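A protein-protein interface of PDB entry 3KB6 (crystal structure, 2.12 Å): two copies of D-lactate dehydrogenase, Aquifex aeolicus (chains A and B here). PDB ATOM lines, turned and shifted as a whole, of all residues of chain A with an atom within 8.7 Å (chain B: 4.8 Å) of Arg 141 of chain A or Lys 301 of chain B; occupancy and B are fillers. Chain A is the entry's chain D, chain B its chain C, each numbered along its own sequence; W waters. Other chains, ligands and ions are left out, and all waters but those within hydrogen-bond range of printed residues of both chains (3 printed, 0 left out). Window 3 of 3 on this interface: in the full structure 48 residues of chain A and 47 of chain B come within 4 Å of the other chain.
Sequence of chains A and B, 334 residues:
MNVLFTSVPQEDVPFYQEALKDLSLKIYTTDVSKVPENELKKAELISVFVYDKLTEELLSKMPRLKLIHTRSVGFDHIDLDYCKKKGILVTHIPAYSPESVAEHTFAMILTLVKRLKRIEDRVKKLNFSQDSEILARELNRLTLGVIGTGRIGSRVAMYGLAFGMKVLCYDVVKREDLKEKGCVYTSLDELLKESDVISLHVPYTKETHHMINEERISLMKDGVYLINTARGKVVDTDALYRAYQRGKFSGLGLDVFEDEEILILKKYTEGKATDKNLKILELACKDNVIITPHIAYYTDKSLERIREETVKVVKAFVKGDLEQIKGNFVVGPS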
ATOM      1  N   VAL A 113      22.934  -9.730  17.760  1.00  0.00           N
ATOM      2  CA  VAL A 113      23.207  -9.963  16.339  1.00  0.00           C
ATOM      3  C   VAL A 113      21.987  -9.528  15.524  1.00  0.00           C
ATOM      4  O   VAL A 113      22.121  -9.035  14.409  1.00  0.00           O
ATOM      5  CB  VAL A 113      23.533 -11.458  16.073  1.00  0.00           C
ATOM      6  CG1 VAL A 113      23.527 -11.746  14.592  1.00  0.00           C
ATOM      7  CG2 VAL A 113      24.900 -11.804  16.696  1.00  0.00           C
ATOM      8  N   LYS A 114      20.800  -9.703  16.087  1.00  0.00           N
ATOM      9  CA  LYS A 114      19.558  -9.238  15.428  1.00  0.00           C
ATOM     10  C   LYS A 114      19.215  -7.746  15.692  1.00  0.00           C
ATOM     11  O   LYS A 114      18.207  -7.216  15.176  1.00  0.00           O
ATOM     12  CB  LYS A 114      18.389 -10.169  15.794  1.00  0.00           C
ATOM     13  CG  LYS A 114      18.562 -11.649  15.288  1.00  0.00           C
ATOM     14  CD  LYS A 114      19.274 -11.748  13.931  1.00  0.00           C
ATOM     15  CE  LYS A 114      19.570 -13.259  13.457  1.00  0.00           C
ATOM     16  NZ  LYS A 114      20.006 -13.440  11.930  1.00  0.00           N
ATOM     17  N   LEU A 135      20.483  -3.399   9.660  1.00  0.00           N
ATOM     18  CA  LEU A 135      20.829  -4.583   8.871  1.00  0.00           C
ATOM     19  C   LEU A 135      21.506  -5.621   9.773  1.00  0.00           C
ATOM     20  O   LEU A 135      22.499  -5.324  10.388  1.00  0.00           O
ATOM     21  CB  LEU A 135      21.748  -4.220   7.700  1.00  0.00           C
ATOM     22  CG  LEU A 135      22.027  -5.382   6.723  1.00  0.00           C
ATOM     23  CD1 LEU A 135      20.727  -5.934   6.127  1.00  0.00           C
ATOM     24  CD2 LEU A 135      23.025  -5.000   5.599  1.00  0.00           C
ATOM     25  N   ALA A 136      20.925  -6.819   9.868  1.00  0.00           N
ATOM     26  CA  ALA A 136      21.394  -7.851  10.780  1.00  0.00           C
ATOM     27  C   ALA A 136      22.432  -8.772  10.117  1.00  0.00           C
ATOM     28  O   ALA A 136      22.652  -8.749   8.897  1.00  0.00           O
ATOM     29  CB  ALA A 136      20.216  -8.658  11.312  1.00  0.00           C
ATOM     30  N   ARG A 137      23.084  -9.558  10.951  1.00  0.00           N
ATOM     31  CA  ARG A 137      23.950 -10.630  10.484  1.00  0.00           C
ATOM     32  C   ARG A 137      23.305 -11.964  10.799  1.00  0.00           C
ATOM     33  O   ARG A 137      22.335 -12.018  11.553  1.00  0.00           O
ATOM     34  CB  ARG A 137      25.342 -10.455  11.093  1.00  0.00           C
ATOM     35  CG  ARG A 137      26.007  -9.181  10.595  1.00  0.00           C
ATOM     36  CD  ARG A 137      27.340  -8.876  11.253  1.00  0.00           C
ATOM     37  NE  ARG A 137      28.391  -9.729  10.710  1.00  0.00           N
ATOM     38  CZ  ARG A 137      29.566  -9.957  11.289  1.00  0.00           C
ATOM     39  NH1 ARG A 137      29.883  -9.398  12.458  1.00  0.00           N
ATOM     40  NH2 ARG A 137      30.426 -10.772  10.699  1.00  0.00           N
ATOM     41  N   GLU A 138      23.793 -13.045  10.194  1.00  0.00           N
ATOM     42  CA  GLU A 138      23.294 -14.412  10.550  1.00  0.00           C
ATOM     43  C   GLU A 138      24.309 -15.235  11.328  1.00  0.00           C
ATOM     44  O   GLU A 138      25.482 -15.255  10.996  1.00  0.00           O
ATOM     45  CB  GLU A 138      22.875 -15.175   9.286  1.00  0.00           C
ATOM     46  CG  GLU A 138      21.931 -14.381   8.359  1.00  0.00           C
ATOM     47  CD  GLU A 138      21.262 -15.230   7.275  1.00  0.00           C
ATOM     48  OE1 GLU A 138      21.465 -16.468   7.261  1.00  0.00           O
ATOM     49  OE2 GLU A 138      20.526 -14.643   6.433  1.00  0.00           O
ATOM     50  N   LEU A 139      23.837 -15.924  12.353  1.00  0.00           N
ATOM     51  CA  LEU A 139      24.656 -16.797  13.163  1.00  0.00           C
ATOM     52  C   LEU A 139      25.289 -17.883  12.313  1.00  0.00           C
ATOM     53  O   LEU A 139      26.451 -18.164  12.481  1.00  0.00           O
ATOM     54  CB  LEU A 139      23.844 -17.463  14.265  1.00  0.00           C
ATOM     55  CG  LEU A 139      23.251 -16.553  15.325  1.00  0.00           C
ATOM     56  CD1 LEU A 139      22.518 -17.414  16.390  1.00  0.00           C
ATOM     57  CD2 LEU A 139      24.329 -15.690  15.942  1.00  0.00           C
ATOM     58  N   ASN A 140      24.545 -18.474  11.376  1.00  0.00           N
ATOM     59  CA  ASN A 140      25.138 -19.529  10.516  1.00  0.00           C
ATOM     60  C   ASN A 140      26.349 -19.060   9.696  1.00  0.00           C
ATOM     61  O   ASN A 140      27.079 -19.883   9.146  1.00  0.00           O
ATOM     62  CB  ASN A 140      24.097 -20.185   9.598  1.00  0.00           C
ATOM     63  CG  ASN A 140      23.519 -19.220   8.601  1.00  0.00           C
ATOM     64  OD1 ASN A 140      24.083 -18.995   7.531  1.00  0.00           O
ATOM     65  ND2 ASN A 140      22.377 -18.648   8.941  1.00  0.00           N
ATOM     66  N   ARG A 141      26.570 -17.749   9.619  1.00  0.00           N
ATOM     67  CA  ARG A 141      27.767 -17.230   8.938  1.00  0.00           C
ATOM     68  C   ARG A 141      28.861 -16.850   9.936  1.00  0.00           C
ATOM     69  O   ARG A 141      29.841 -16.261   9.569  1.00  0.00           O
ATOM     70  CB  ARG A 141      27.445 -16.010   8.070  1.00  0.00           C
ATOM     71  CG  ARG A 141      26.459 -16.295   6.944  1.00  0.00           C
ATOM     72  CD  ARG A 141      27.146 -17.054   5.815  1.00  0.00           C
ATOM     73  NE  ARG A 141      26.548 -16.793   4.507  1.00  0.00           N
ATOM     74  CZ  ARG A 141      27.015 -17.279   3.359  1.00  0.00           C
ATOM     75  NH1 ARG A 141      28.096 -18.045   3.343  1.00  0.00           N
ATOM     76  NH2 ARG A 141      26.396 -16.995   2.218  1.00  0.00           N
ATOM     77  N   LEU A 142      28.691 -17.170  11.209  1.00  0.00           N
ATOM     78  CA  LEU A 142      29.652 -16.701  12.170  1.00  0.00           C
ATOM     79  C   LEU A 142      30.368 -17.858  12.865  1.00  0.00           C
ATOM     80  O   LEU A 142      29.909 -19.000  12.829  1.00  0.00           O
ATOM     81  CB  LEU A 142      28.986 -15.804  13.194  1.00  0.00           C
ATOM     82  CG  LEU A 142      28.313 -14.529  12.678  1.00  0.00           C
ATOM     83  CD1 LEU A 142      27.671 -13.777  13.856  1.00  0.00           C
ATOM     84  CD2 LEU A 142      29.256 -13.652  11.934  1.00  0.00           C
ATOM     85  N   THR A 143      31.512 -17.497  13.463  1.00  0.00           N
ATOM     86  CA  THR A 143      32.307 -18.358  14.279  1.00  0.00           C
ATOM     87  C   THR A 143      32.104 -17.987  15.726  1.00  0.00           C
ATOM     88  O   THR A 143      32.327 -16.858  16.118  1.00  0.00           O
ATOM     89  CB  THR A 143      33.812 -18.198  13.918  1.00  0.00           C
ATOM     90  OG1 THR A 143      34.027 -18.583  12.533  1.00  0.00           O
ATOM     91  CG2 THR A 143      34.684 -19.031  14.868  1.00  0.00           C
ATOM     92  N   LEU A 144      31.674 -18.950  16.507  1.00  0.00           N
ATOM     93  CA  LEU A 144      31.561 -18.841  17.962  1.00  0.00           C
ATOM     94  C   LEU A 144      32.786 -19.420  18.663  1.00  0.00           C
ATOM     95  O   LEU A 144      33.197 -20.548  18.327  1.00  0.00           O
ATOM     96  CB  LEU A 144      30.349 -19.649  18.411  1.00  0.00           C
ATOM     97  CG  LEU A 144      30.073 -19.692  19.909  1.00  0.00           C
ATOM     98  CD1 LEU A 144      29.758 -18.280  20.454  1.00  0.00           C
ATOM     99  CD2 LEU A 144      28.963 -20.660  20.174  1.00  0.00           C
ATOM    100  N   GLY A 160      25.238 -23.476  19.428  1.00  0.00           N
ATOM    101  CA  GLY A 160      25.890 -22.845  18.297  1.00  0.00           C
ATOM    102  C   GLY A 160      25.991 -23.768  17.088  1.00  0.00           C
ATOM    103  O   GLY A 160      25.810 -23.343  15.930  1.00  0.00           O
ATOM    104  N   PHE A 163      22.750 -23.914  15.317  1.00  0.00           N
ATOM    105  CA  PHE A 163      22.539 -22.728  14.481  1.00  0.00           C
ATOM    106  C   PHE A 163      23.428 -22.679  13.269  1.00  0.00           C
ATOM    107  O   PHE A 163      23.410 -21.703  12.539  1.00  0.00           O
ATOM    108  CB  PHE A 163      22.659 -21.424  15.309  1.00  0.00           C
ATOM    109  CG  PHE A 163      21.420 -21.094  16.065  1.00  0.00           C
ATOM    110  CD1 PHE A 163      20.329 -20.549  15.411  1.00  0.00           C
ATOM    111  CD2 PHE A 163      21.321 -21.329  17.412  1.00  0.00           C
ATOM    112  CE1 PHE A 163      19.177 -20.245  16.072  1.00  0.00           C
ATOM    113  CE2 PHE A 163      20.135 -21.012  18.099  1.00  0.00           C
ATOM    114  CZ  PHE A 163      19.062 -20.493  17.409  1.00  0.00           C
ATOM    115  N   GLY A 164      24.206 -23.723  13.011  1.00  0.00           N
ATOM    116  CA  GLY A 164      25.095 -23.742  11.827  1.00  0.00           C
ATOM    117  C   GLY A 164      26.345 -22.908  11.993  1.00  0.00           C
ATOM    118  O   GLY A 164      27.013 -22.548  11.024  1.00  0.00           O
ATOM    119  N   MET A 165      26.677 -22.561  13.224  1.00  0.00           N
ATOM    120  CA  MET A 165      27.907 -21.829  13.436  1.00  0.00           C
ATOM    121  C   MET A 165      29.112 -22.751  13.440  1.00  0.00           C
ATOM    122  O   MET A 165      29.023 -23.909  13.842  1.00  0.00           O
ATOM    123  CB  MET A 165      27.866 -21.074  14.740  1.00  0.00           C
ATOM    124  CG  MET A 165      27.108 -19.808  14.631  1.00  0.00           C
ATOM    125  SD  MET A 165      27.007 -19.025  16.340  1.00  0.00           S
ATOM    126  CE  MET A 165      25.429 -19.961  16.909  1.00  0.00           C
ATOM    127  N   LYS A 166      30.237 -22.243  12.943  1.00  0.00           N
ATOM    128  CA  LYS A 166      31.543 -22.845  13.270  1.00  0.00           C
ATOM    129  C   LYS A 166      31.823 -22.549  14.752  1.00  0.00           C
ATOM    130  O   LYS A 166      31.798 -21.381  15.174  1.00  0.00           O
ATOM    131  CB  LYS A 166      32.665 -22.238  12.441  1.00  0.00           C
ATOM    132  CG  LYS A 166      33.944 -23.024  12.617  1.00  0.00           C
ATOM    133  CD  LYS A 166      35.127 -22.440  11.876  1.00  0.00           C
ATOM    134  CE  LYS A 166      36.262 -23.499  11.843  1.00  0.00           C
ATOM    135  NZ  LYS A 166      37.544 -22.945  11.345  1.00  0.00           N
ATOM    136  N   GLU A 194      40.028 -15.598  15.910  1.00  0.00           N
ATOM    137  CA  GLU A 194      39.197 -16.115  14.826  1.00  0.00           C
ATOM    138  C   GLU A 194      37.704 -16.034  15.131  1.00  0.00           C
ATOM    139  O   GLU A 194      36.917 -16.203  14.228  1.00  0.00           O
ATOM    140  CB  GLU A 194      39.563 -17.576  14.486  1.00  0.00           C
ATOM    141  CG  GLU A 194      41.013 -17.799  13.974  1.00  0.00           C
ATOM    142  CD  GLU A 194      41.203 -17.482  12.471  1.00  0.00           C
ATOM    143  OE1 GLU A 194      40.433 -16.681  11.895  1.00  0.00           O
ATOM    144  OE2 GLU A 194      42.141 -18.048  11.864  1.00  0.00           O
ATOM    145  N   ASP A 196      33.952 -14.608  15.869  1.00  0.00           N
ATOM    146  CA  ASP A 196      33.116 -13.422  15.667  1.00  0.00           C
ATOM    147  C   ASP A 196      32.302 -13.125  16.933  1.00  0.00           C
ATOM    148  O   ASP A 196      31.993 -11.959  17.204  1.00  0.00           O
ATOM    149  CB  ASP A 196      32.181 -13.620  14.481  1.00  0.00           C
ATOM    150  CG  ASP A 196      32.921 -13.876  13.169  1.00  0.00           C
ATOM    151  OD1 ASP A 196      33.746 -13.034  12.773  1.00  0.00           O
ATOM    152  OD2 ASP A 196      32.653 -14.924  12.528  1.00  0.00           O
ATOM    153  N   VAL A 197      31.970 -14.176  17.680  1.00  0.00           N
ATOM    154  CA  VAL A 197      31.264 -14.123  18.968  1.00  0.00           C
ATOM    155  C   VAL A 197      32.045 -14.958  19.973  1.00  0.00           C
ATOM    156  O   VAL A 197      32.379 -16.135  19.704  1.00  0.00           O
ATOM    157  CB  VAL A 197      29.831 -14.728  18.879  1.00  0.00           C
ATOM    158  CG1 VAL A 197      29.115 -14.630  20.210  1.00  0.00           C
ATOM    159  CG2 VAL A 197      28.990 -14.050  17.764  1.00  0.00           C
ATOM    160  N   LYS A 221      38.869  -9.768  16.904  1.00  0.00           N
ATOM    161  CA  LYS A 221      38.571  -9.012  15.691  1.00  0.00           C
ATOM    162  C   LYS A 221      37.916  -7.715  16.108  1.00  0.00           C
ATOM    163  O   LYS A 221      37.167  -7.692  17.083  1.00  0.00           O
ATOM    164  CB  LYS A 221      37.555  -9.746  14.797  1.00  0.00           C
ATOM    165  CG  LYS A 221      38.049 -11.025  14.170  1.00  0.00           C
ATOM    166  CD  LYS A 221      36.893 -11.768  13.509  1.00  0.00           C
ATOM    167  CE  LYS A 221      37.377 -12.989  12.774  1.00  0.00           C
ATOM    168  NZ  LYS A 221      36.264 -13.701  12.085  1.00  0.00           N
ATOM    169  N   TYR B  96      16.330 -17.498  -0.540  1.00  0.00           N
ATOM    170  CA  TYR B  96      17.509 -16.633  -0.332  1.00  0.00           C
ATOM    171  C   TYR B  96      18.069 -16.843   1.100  1.00  0.00           C
ATOM    172  O   TYR B  96      19.263 -16.891   1.282  1.00  0.00           O
ATOM    173  CB  TYR B  96      17.197 -15.152  -0.619  1.00  0.00           C
ATOM    174  CG  TYR B  96      16.046 -14.581   0.186  1.00  0.00           C
ATOM    175  CD1 TYR B  96      16.235 -14.197   1.508  1.00  0.00           C
ATOM    176  CD2 TYR B  96      14.771 -14.449  -0.367  1.00  0.00           C
ATOM    177  CE1 TYR B  96      15.198 -13.706   2.266  1.00  0.00           C
ATOM    178  CE2 TYR B  96      13.720 -13.942   0.378  1.00  0.00           C
ATOM    179  CZ  TYR B  96      13.947 -13.568   1.705  1.00  0.00           C
ATOM    180  OH  TYR B  96      12.951 -13.088   2.484  1.00  0.00           O
ATOM    181  N   SER B  97      17.200 -17.006   2.103  1.00  0.00           N
ATOM    182  CA  SER B  97      17.671 -17.236   3.466  1.00  0.00           C
ATOM    183  C   SER B  97      16.554 -17.583   4.395  1.00  0.00           C
ATOM    184  O   SER B  97      16.092 -16.736   5.167  1.00  0.00           O
ATOM    185  CB  SER B  97      18.428 -16.019   4.043  1.00  0.00           C
ATOM    186  OG  SER B  97      18.916 -16.304   5.364  1.00  0.00           O
ATOM    187  N   GLU B  99      17.160 -19.208   6.937  1.00  0.00           N
ATOM    188  CA  GLU B  99      17.817 -19.115   8.269  1.00  0.00           C
ATOM    189  C   GLU B  99      17.605 -17.737   8.913  1.00  0.00           C
ATOM    190  O   GLU B  99      17.407 -17.627  10.099  1.00  0.00           O
ATOM    191  CB  GLU B  99      19.322 -19.385   8.180  1.00  0.00           C
ATOM    192  CG  GLU B  99      19.682 -20.791   7.746  1.00  0.00           C
ATOM    193  CD  GLU B  99      19.675 -20.988   6.227  1.00  0.00           C
ATOM    194  OE1 GLU B  99      19.438 -20.044   5.439  1.00  0.00           O
ATOM    195  OE2 GLU B  99      19.896 -22.131   5.819  1.00  0.00           O
ATOM    196  N   THR B 299      18.887  -9.353   6.641  1.00  0.00           N
ATOM    197  CA  THR B 299      20.273  -9.686   7.000  1.00  0.00           C
ATOM    198  C   THR B 299      21.123  -9.434   5.786  1.00  0.00           C
ATOM    199  O   THR B 299      20.598  -9.441   4.682  1.00  0.00           O
ATOM    200  CB  THR B 299      20.414 -11.151   7.411  1.00  0.00           C
ATOM    201  OG1 THR B 299      20.251 -11.967   6.261  1.00  0.00           O
ATOM    202  CG2 THR B 299      19.381 -11.564   8.445  1.00  0.00           C
ATOM    203  N   ASP B 300      22.418  -9.155   5.970  1.00  0.00           N
ATOM    204  CA  ASP B 300      23.347  -8.935   4.846  1.00  0.00           C
ATOM    205  C   ASP B 300      23.398 -10.088   3.814  1.00  0.00           C
ATOM    206  O   ASP B 300      23.471  -9.847   2.624  1.00  0.00           O
ATOM    207  CB  ASP B 300      24.757  -8.608   5.340  1.00  0.00           C
ATOM    208  CG  ASP B 300      25.344  -9.683   6.302  1.00  0.00           C
ATOM    209  OD1 ASP B 300      24.698 -10.686   6.686  1.00  0.00           O
ATOM    210  OD2 ASP B 300      26.503  -9.483   6.698  1.00  0.00           O
ATOM    211  N   LYS B 301      23.338 -11.324   4.276  1.00  0.00           N
ATOM    212  CA  LYS B 301      23.334 -12.467   3.365  1.00  0.00           C
ATOM    213  C   LYS B 301      22.029 -12.489   2.538  1.00  0.00           C
ATOM    214  O   LYS B 301      22.071 -12.715   1.333  1.00  0.00           O
ATOM    215  CB  LYS B 301      23.494 -13.761   4.153  1.00  0.00           C
ATOM    216  CG  LYS B 301      23.528 -15.044   3.319  1.00  0.00           C
ATOM    217  CD  LYS B 301      23.206 -16.295   4.169  1.00  0.00           C
ATOM    218  CE  LYS B 301      21.819 -16.898   3.856  1.00  0.00           C
ATOM    219  NZ  LYS B 301      21.334 -17.959   4.881  1.00  0.00           N
ATOM    220  N   SER B 302      20.885 -12.264   3.186  1.00  0.00           N
ATOM    221  CA  SER B 302      19.615 -12.152   2.457  1.00  0.00           C
ATOM    222  C   SER B 302      19.673 -11.138   1.331  1.00  0.00           C
ATOM    223  O   SER B 302      19.255 -11.454   0.222  1.00  0.00           O
ATOM    224  CB  SER B 302      18.441 -11.776   3.369  1.00  0.00           C
ATOM    225  OG  SER B 302      18.030 -12.834   4.213  1.00  0.00           O
ATOM    226  N   LEU B 303      20.176  -9.928   1.607  1.00  0.00           N
ATOM    227  CA  LEU B 303      20.181  -8.854   0.595  1.00  0.00           C
ATOM    228  C   LEU B 303      21.095  -9.191  -0.559  1.00  0.00           C
ATOM    229  O   LEU B 303      20.709  -9.029  -1.707  1.00  0.00           O
ATOM    230  CB  LEU B 303      20.548  -7.479   1.185  1.00  0.00           C
ATOM    231  CG  LEU B 303      19.597  -6.951   2.280  1.00  0.00           C
ATOM    232  CD1 LEU B 303      19.908  -5.491   2.645  1.00  0.00           C
ATOM    233  CD2 LEU B 303      18.098  -7.138   1.909  1.00  0.00           C
ATOM    234  N   GLU B 304      22.283  -9.726  -0.263  1.00  0.00           N
ATOM    235  CA  GLU B 304      23.175 -10.218  -1.301  1.00  0.00           C
ATOM    236  C   GLU B 304      22.497 -11.277  -2.188  1.00  0.00           C
ATOM    237  O   GLU B 304      22.534 -11.183  -3.421  1.00  0.00           O
ATOM    238  CB  GLU B 304      24.430 -10.810  -0.675  1.00  0.00           C
ATOM    239  CG  GLU B 304      25.485 -11.220  -1.675  1.00  0.00           C
ATOM    240  CD  GLU B 304      26.794 -11.681  -1.006  1.00  0.00           C
ATOM    241  OE1 GLU B 304      26.855 -11.706   0.255  1.00  0.00           O
ATOM    242  OE2 GLU B 304      27.751 -12.026  -1.751  1.00  0.00           O
ATOM    243  N   ARG B 305      21.884 -12.274  -1.570  1.00  0.00           N
ATOM    244  CA  ARG B 305      21.282 -13.354  -2.353  1.00  0.00           C
ATOM    245  C   ARG B 305      20.059 -12.891  -3.177  1.00  0.00           C
ATOM    246  O   ARG B 305      19.846 -13.390  -4.277  1.00  0.00           O
ATOM    247  CB  ARG B 305      20.867 -14.516  -1.459  1.00  0.00           C
ATOM    248  CG  ARG B 305      22.030 -15.178  -0.679  1.00  0.00           C
ATOM    249  CD  ARG B 305      22.801 -16.219  -1.501  1.00  0.00           C
ATOM    250  NE  ARG B 305      21.918 -17.269  -2.028  1.00  0.00           N
ATOM    251  CZ  ARG B 305      21.596 -17.448  -3.320  1.00  0.00           C
ATOM    252  NH1 ARG B 305      22.088 -16.669  -4.289  1.00  0.00           N
ATOM    253  NH2 ARG B 305      20.772 -18.445  -3.651  1.00  0.00           N
HETATM  254  O   HOH W   1      27.871 -11.537   8.512  1.00  0.00           O
HETATM  255  O   HOH W   2      23.600 -19.477   4.929  1.00  0.00           O
HETATM  256  O   HOH W   3      25.770 -12.769   8.008  1.00  0.00           O
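Leu 135 of chain A touches Thr 299 of chain B (CD1 to C, 3.5 Å).
Leu 135 of chain A touches Asp 300 of chain B.
CD1 of Leu 135 of chain A touches CD1 of Leu 303 of chain B, 3.6 Å away.
Ala 136 of chain A touches Thr 299 of chain B.
OD1 of Asp 300 of chain B touches CA of Arg 137 of chain A (3.9 Å).
CB of Glu 99 of chain B touches OE1 of Glu 138 of chain A (3.7 Å).
OE2 of Glu 138 of chain A touches OG of Ser 302 of chain B, at 3.8 Å.
ND2 of Asn 140 of chain A touches CB of Glu 99 of chain B, at 3.2 Å.
OD1 of Asn 140 of chain A touches NZ of Lys 301 of chain B, at 3.96 Å.
Lys 301 of chain B touches Arg 141 of chain A.
Water W2 lies within hydrogen-bond range of OD1 of Asn 140 of chain A and NZ of Lys 301 of chain B.
Water W3 bridges OD1 of Asp 300 of chain B and N of Glu 138 of chain A.
Water W1 bridges NE of Arg 137 of chain A and OD2 of Asp 300 of chain B.
The side-chain hydroxyl (OG) of Ser 97 of chain B is in hydrogen-bond range of the side-chain amino group (NZ) of Lys 301 of chain B.
The side-chain carboxylate (OE1) of Glu 99 of chain B lies within salt-bridge range of the side-chain amino group (NZ) of Lys 301 of chain B (2.9 Å).
The side-chain hydroxyl (OG1) of Thr 299 of chain B sits at hydrogen-bond distance from the side-chain hydroxyl (OG) of Ser 302 of chain B (3.1 Å).
NZ of Lys 114 of chain A sits at hydrogen-bond distance from O of Arg 137 of chain A (2.8 Å).
The side-chain amide nitrogen (ND2) of Asn 140 of chain A sits at hydrogen-bond distance from the side-chain carboxylate (OE1) of Glu 138 of chain A, 2.9 Å away.
Of the printed residues of chain B, Leu 135 of chain A touches Thr 299 (3.5 Å), Asp 300 (3.6 Å) and Leu 303 (3.6 Å).
Printed residues of chain B within 4 Å of Glu 138 of chain A: Ser 97 (2.5 Å), Glu 99 (3.7 Å), Thr 299 (2.7 Å), Lys 301 (2.8 Å) and Ser 302 (3.8 Å).
Arg 141 of chain A touches just one residue of chain B: Lys 301 (3.4 Å).
Of the printed residues of chain A, Glu 99 of chain B touches Glu 138 (3.7 Å) and Asn 140 (3.2 Å).
Of the printed residues of chain A, Ser 302 of chain B touches Glu 138.
Printed residues of chain A within 4 Å of Leu 303 of chain B: Leu 135.
The nearest printed residue of chain B that does not touch Arg 141 of chain A is Arg 305 of chain B (5.2 Å).
The nearest printed residue of chain B that does not touch Leu 135 of chain A is Lys 301 of chain B (6.3 Å).
Of the 10 printed residues of chain B, 7 touch a printed residue of chain A.
Printed residues of chain B that touch a printed residue of chain A: Ser 97, Glu 99, Thr 299, Asp 300, Lys 301, Ser 302 and Leu 303.
Hydrophobic or aromatic side chains of chain B that line the printed part of chain A: Leu 303.
Among the printed residues, Asp or Glu carboxylates within 4 Å of a Lys or Arg side-chain nitrogen of the other chain: Glu 138 of chain A with Lys 301 of chain B (2.8 Å).
The side-chain carboxylate (OE2) of Glu 138 of chain A sits at hydrogen-bond distance from the side-chain hydroxyl (OG) of Ser 97 of chain B (2.5 Å).
The side-chain hydroxyl (OG1) of Thr 299 of chain B is in hydrogen-bond range of the side-chain carboxylate (OE2) of Glu 138 of chain A, 2.7 Å away.
N of Asp 300 of chain B is in hydrogen-bond range of O of Ala 136 of chain A, at 3.0 Å.
The side-chain carboxylate (OE1) of Glu 138 of chain A is in salt-bridge range of the side-chain amino group (NZ) of Lys 301 of chain B (2.8 Å).
No position is printed for both chains.
Of the 14 pairs that touch across the chains among the printed residues, none has its exchanged pair printed and touching as well.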
